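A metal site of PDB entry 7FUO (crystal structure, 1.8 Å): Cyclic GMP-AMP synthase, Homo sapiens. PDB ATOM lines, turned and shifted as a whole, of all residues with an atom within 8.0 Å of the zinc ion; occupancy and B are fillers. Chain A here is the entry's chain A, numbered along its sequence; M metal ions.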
ATOM      1  N   LEU A 227       8.052 -21.183 -20.133  1.00  0.00           N
ATOM      2  CA  LEU A 227       7.519 -22.161 -19.192  1.00  0.00           C
ATOM      3  C   LEU A 227       7.123 -23.461 -19.882  1.00  0.00           C
ATOM      4  O   LEU A 227       7.217 -24.536 -19.280  1.00  0.00           O
ATOM      5  CB  LEU A 227       6.324 -21.588 -18.440  1.00  0.00           C
ATOM      6  CG  LEU A 227       6.658 -20.614 -17.317  1.00  0.00           C
ATOM      7  CD1 LEU A 227       5.390 -20.196 -16.619  1.00  0.00           C
ATOM      8  CD2 LEU A 227       7.589 -21.289 -16.329  1.00  0.00           C
ATOM      9  N   ASN A 229       8.709 -24.824 -22.335  1.00  0.00           N
ATOM     10  CA  ASN A 229       9.884 -25.404 -22.967  1.00  0.00           C
ATOM     11  C   ASN A 229      11.063 -24.956 -22.119  1.00  0.00           C
ATOM     12  O   ASN A 229      11.940 -24.215 -22.555  1.00  0.00           O
ATOM     13  CB  ASN A 229       9.992 -24.928 -24.422  1.00  0.00           C
ATOM     14  CG  ASN A 229      10.712 -25.921 -25.322  1.00  0.00           C
ATOM     15  OD1 ASN A 229      11.194 -27.004 -24.892  1.00  0.00           O
ATOM     16  ND2 ASN A 229      10.798 -25.562 -26.604  1.00  0.00           N
ATOM     17  N   HIS A 230      11.063 -25.359 -20.856  1.00  0.00           N
ATOM     18  CA  HIS A 230      11.834 -24.712 -19.805  1.00  0.00           C
ATOM     19  C   HIS A 230      13.138 -25.417 -19.463  1.00  0.00           C
ATOM     20  O   HIS A 230      13.928 -24.879 -18.678  1.00  0.00           O
ATOM     21  CB  HIS A 230      11.000 -24.618 -18.514  1.00  0.00           C
ATOM     22  CG  HIS A 230      10.575 -25.952 -17.966  1.00  0.00           C
ATOM     23  ND1 HIS A 230       9.258 -26.315 -17.862  1.00  0.00           N
ATOM     24  CD2 HIS A 230      11.289 -27.014 -17.527  1.00  0.00           C
ATOM     25  CE1 HIS A 230       9.168 -27.547 -17.377  1.00  0.00           C
ATOM     26  NE2 HIS A 230      10.389 -27.989 -17.163  1.00  0.00           N
ATOM     27  N   GLY A 231      13.382 -26.591 -19.981  1.00  0.00           N
ATOM     28  CA  GLY A 231      14.550 -27.329 -19.568  1.00  0.00           C
ATOM     29  C   GLY A 231      15.722 -27.061 -20.449  1.00  0.00           C
ATOM     30  O   GLY A 231      15.587 -26.677 -21.606  1.00  0.00           O
ATOM     31  N   LYS A 232      16.916 -27.258 -19.916  1.00  0.00           N
ATOM     32  CA  LYS A 232      18.023 -27.504 -20.805  1.00  0.00           C
ATOM     33  C   LYS A 232      17.751 -28.746 -21.651  1.00  0.00           C
ATOM     34  O   LYS A 232      18.089 -28.781 -22.828  1.00  0.00           O
ATOM     35  CB  LYS A 232      19.334 -27.657 -20.046  1.00  0.00           C
ATOM     36  CG  LYS A 232      20.514 -27.851 -20.977  1.00  0.00           C
ATOM     37  CD  LYS A 232      21.845 -27.685 -20.241  1.00  0.00           C
ATOM     38  CE  LYS A 232      22.055 -26.260 -19.782  1.00  0.00           C
ATOM     39  NZ  LYS A 232      21.900 -25.275 -20.899  1.00  0.00           N
ATOM     40  N   SER A 233      17.110 -29.765 -21.064  1.00  0.00           N
ATOM     41  CA  SER A 233      16.726 -30.936 -21.843  1.00  0.00           C
ATOM     42  C   SER A 233      15.443 -30.656 -22.619  1.00  0.00           C
ATOM     43  O   SER A 233      14.467 -30.122 -22.083  1.00  0.00           O
ATOM     44  CB  SER A 233      16.505 -32.144 -20.949  1.00  0.00           C
ATOM     45  OG  SER A 233      15.938 -33.217 -21.690  1.00  0.00           O
ATOM     46  N   THR A 235      13.316 -32.757 -23.382  1.00  0.00           N
ATOM     47  CA  THR A 235      12.294 -33.649 -22.837  1.00  0.00           C
ATOM     48  C   THR A 235      12.078 -33.420 -21.338  1.00  0.00           C
ATOM     49  O   THR A 235      11.520 -34.294 -20.669  1.00  0.00           O
ATOM     50  CB  THR A 235      12.668 -35.103 -23.077  1.00  0.00           C
ATOM     51  OG1 THR A 235      14.027 -35.311 -22.677  1.00  0.00           O
ATOM     52  CG2 THR A 235      12.590 -35.434 -24.555  1.00  0.00           C
ATOM     53  N   CYS A 236      12.524 -32.286 -20.806  1.00  0.00           N
ATOM     54  CA  CYS A 236      12.348 -32.001 -19.393  1.00  0.00           C
ATOM     55  C   CYS A 236      10.867 -31.969 -19.054  1.00  0.00           C
ATOM     56  O   CYS A 236      10.097 -31.251 -19.696  1.00  0.00           O
ATOM     57  CB  CYS A 236      13.001 -30.666 -19.034  1.00  0.00           C
ATOM     58  SG  CYS A 236      13.018 -30.256 -17.269  1.00  0.00           S
ATOM     59  N   CYS A 237      10.492 -32.736 -18.025  1.00  0.00           N
ATOM     60  CA  CYS A 237       9.124 -32.886 -17.553  1.00  0.00           C
ATOM     61  C   CYS A 237       8.243 -33.592 -18.582  1.00  0.00           C
ATOM     62  O   CYS A 237       7.031 -33.384 -18.613  1.00  0.00           O
ATOM     63  CB  CYS A 237       8.509 -31.555 -17.135  1.00  0.00           C
ATOM     64  SG  CYS A 237       9.322 -30.802 -15.711  1.00  0.00           S
ATOM     65  N   GLU A 238       8.830 -34.436 -19.431  1.00  0.00           N
ATOM     66  CA  GLU A 238       8.050 -35.200 -20.401  1.00  0.00           C
ATOM     67  C   GLU A 238       8.174 -36.709 -20.218  1.00  0.00           C
ATOM     68  O   GLU A 238       7.698 -37.465 -21.073  1.00  0.00           O
ATOM     69  CB  GLU A 238       8.438 -34.794 -21.831  1.00  0.00           C
ATOM     70  CG  GLU A 238       8.283 -33.297 -22.042  1.00  0.00           C
ATOM     71  CD  GLU A 238       8.387 -32.846 -23.510  1.00  0.00           C
ATOM     72  OE1 GLU A 238       8.310 -33.706 -24.429  1.00  0.00           O
ATOM     73  OE2 GLU A 238       8.533 -31.609 -23.726  1.00  0.00           O
ATOM     74  N   GLU A 242      12.639 -37.395 -15.695  1.00  0.00           N
ATOM     75  CA  GLU A 242      13.030 -35.992 -15.884  1.00  0.00           C
ATOM     76  C   GLU A 242      11.934 -35.097 -15.331  1.00  0.00           C
ATOM     77  O   GLU A 242      11.281 -34.356 -16.065  1.00  0.00           O
ATOM     78  CB  GLU A 242      13.266 -35.659 -17.355  1.00  0.00           C
ATOM     79  CG  GLU A 242      14.361 -36.400 -18.040  1.00  0.00           C
ATOM     80  CD  GLU A 242      14.548 -35.904 -19.452  1.00  0.00           C
ATOM     81  OE1 GLU A 242      15.087 -34.792 -19.618  1.00  0.00           O
ATOM     82  OE2 GLU A 242      14.125 -36.630 -20.377  1.00  0.00           O
ATOM     83  N   LYS A 243      11.738 -35.146 -14.030  1.00  0.00           N
ATOM     84  CA  LYS A 243      10.788 -34.281 -13.348  1.00  0.00           C
ATOM     85  C   LYS A 243      11.570 -33.184 -12.627  1.00  0.00           C
ATOM     86  O   LYS A 243      12.403 -33.480 -11.763  1.00  0.00           O
ATOM     87  CB  LYS A 243       9.911 -35.114 -12.421  1.00  0.00           C
ATOM     88  CG  LYS A 243       8.921 -35.990 -13.185  1.00  0.00           C
ATOM     89  CD  LYS A 243       7.963 -35.043 -13.906  1.00  0.00           C
ATOM     90  CE  LYS A 243       7.069 -35.722 -14.921  1.00  0.00           C
ATOM     91  NZ  LYS A 243       6.130 -34.691 -15.474  1.00  0.00           N
ATOM     92  N   CYS A 244      11.365 -31.924 -13.031  1.00  0.00           N
ATOM     93  CA  CYS A 244      12.020 -30.758 -12.426  1.00  0.00           C
ATOM     94  C   CYS A 244      11.003 -29.966 -11.636  1.00  0.00           C
ATOM     95  O   CYS A 244       9.801 -30.248 -11.668  1.00  0.00           O
ATOM     96  CB  CYS A 244      12.740 -29.897 -13.475  1.00  0.00           C
ATOM     97  SG  CYS A 244      11.772 -28.572 -14.241  1.00  0.00           S
ATOM     98  N   CYS A 245      11.478 -28.984 -10.866  1.00  0.00           N
ATOM     99  CA  CYS A 245      10.575 -28.206 -10.025  1.00  0.00           C
ATOM    100  C   CYS A 245      10.620 -26.713 -10.348  1.00  0.00           C
ATOM    101  O   CYS A 245      10.389 -25.873  -9.481  1.00  0.00           O
ATOM    102  CB  CYS A 245      10.882 -28.445  -8.544  1.00  0.00           C
ATOM    103  SG  CYS A 245      12.561 -28.010  -8.031  1.00  0.00           S
ATOM    104  N   ARG A 246      10.909 -26.360 -11.606  1.00  0.00           N
ATOM    105  CA  ARG A 246      10.928 -24.955 -11.969  1.00  0.00           C
ATOM    106  C   ARG A 246       9.545 -24.332 -11.843  1.00  0.00           C
ATOM    107  O   ARG A 246       9.378 -23.276 -11.222  1.00  0.00           O
ATOM    108  CB  ARG A 246      11.475 -24.778 -13.369  1.00  0.00           C
ATOM    109  CG  ARG A 246      12.951 -24.999 -13.513  1.00  0.00           C
ATOM    110  CD  ARG A 246      13.318 -24.854 -14.935  1.00  0.00           C
ATOM    111  NE  ARG A 246      14.743 -24.970 -15.209  1.00  0.00           N
ATOM    112  CZ  ARG A 246      15.361 -26.050 -15.697  1.00  0.00           C
ATOM    113  NH1 ARG A 246      14.699 -27.161 -15.957  1.00  0.00           N
ATOM    114  NH2 ARG A 246      16.656 -26.035 -15.947  1.00  0.00           N
ATOM    115  N   LYS A 247       8.532 -24.955 -12.451  1.00  0.00           N
ATOM    116  CA  LYS A 247       7.185 -24.398 -12.366  1.00  0.00           C
ATOM    117  C   LYS A 247       6.738 -24.292 -10.915  1.00  0.00           C
ATOM    118  O   LYS A 247       6.126 -23.290 -10.523  1.00  0.00           O
ATOM    119  CB  LYS A 247       6.202 -25.239 -13.166  1.00  0.00           C
ATOM    120  CG  LYS A 247       6.434 -25.171 -14.658  1.00  0.00           C
ATOM    121  CD  LYS A 247       5.148 -25.552 -15.402  1.00  0.00           C
ATOM    122  CE  LYS A 247       5.380 -25.584 -16.892  1.00  0.00           C
ATOM    123  NZ  LYS A 247       4.181 -26.038 -17.634  1.00  0.00           N
ATOM    124  N   ASP A 292      19.246 -28.866 -15.671  1.00  0.00           N
ATOM    125  CA  ASP A 292      18.064 -29.528 -15.141  1.00  0.00           C
ATOM    126  C   ASP A 292      18.354 -30.190 -13.804  1.00  0.00           C
ATOM    127  O   ASP A 292      17.457 -30.297 -12.975  1.00  0.00           O
ATOM    128  CB  ASP A 292      17.581 -30.576 -16.129  1.00  0.00           C
ATOM    129  CG  ASP A 292      17.005 -29.978 -17.409  1.00  0.00           C
ATOM    130  OD1 ASP A 292      16.742 -28.753 -17.480  1.00  0.00           O
ATOM    131  OD2 ASP A 292      16.803 -30.783 -18.344  1.00  0.00           O
ATOM    132  N   TRP A 295      17.448 -28.518 -10.547  1.00  0.00           N
ATOM    133  CA  TRP A 295      16.018 -28.300 -10.368  1.00  0.00           C
ATOM    134  C   TRP A 295      15.307 -29.622 -10.141  1.00  0.00           C
ATOM    135  O   TRP A 295      14.122 -29.757 -10.460  1.00  0.00           O
ATOM    136  CB  TRP A 295      15.432 -27.550 -11.568  1.00  0.00           C
ATOM    137  CG  TRP A 295      15.946 -26.170 -11.692  1.00  0.00           C
ATOM    138  CD1 TRP A 295      16.977 -25.759 -12.464  1.00  0.00           C
ATOM    139  CD2 TRP A 295      15.485 -25.016 -10.984  1.00  0.00           C
ATOM    140  NE1 TRP A 295      17.189 -24.411 -12.293  1.00  0.00           N
ATOM    141  CE2 TRP A 295      16.282 -23.925 -11.381  1.00  0.00           C
ATOM    142  CE3 TRP A 295      14.478 -24.798 -10.030  1.00  0.00           C
ATOM    143  CZ2 TRP A 295      16.098 -22.641 -10.887  1.00  0.00           C
ATOM    144  CZ3 TRP A 295      14.296 -23.502  -9.543  1.00  0.00           C
ATOM    145  CH2 TRP A 295      15.097 -22.458  -9.974  1.00  0.00           C
HETATM  146 ZN    ZN M   1      11.072 -29.563 -16.230  1.00  0.00          ZN
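The backbone carbonyl oxygen of Leu 227 lies within hydrogen-bond range of a ring nitrogen (ND1) of His 230 (3.1 Å). N of Cys 237 lies within hydrogen-bond range of O of Glu 242, at 2.7 Å. SG of Cys 236 sits close to NH1 of Arg 246, at 3.8 Å. The side-chain sulfur (SG) of Cys 244 lies close to the backbone NH (N) of Arg 246 (3.5 Å).
The zinc ion is bound by NE2 of His 230, at 2.0 Å. SG of Cys 237 binds the zinc ion, at 2.2 Å. SG of Cys 236 binds the zinc ion. The side-chain sulfur (SG) of Cys 244 binds the zinc ion, at 2.3 Å.
Four residues have an atom within 4 Å of the zinc ion: His 230, Cys 236, Cys 237 and Cys 244. The nearest printed residue that does not touch the zinc ion is Arg 246 (4.4 Å).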
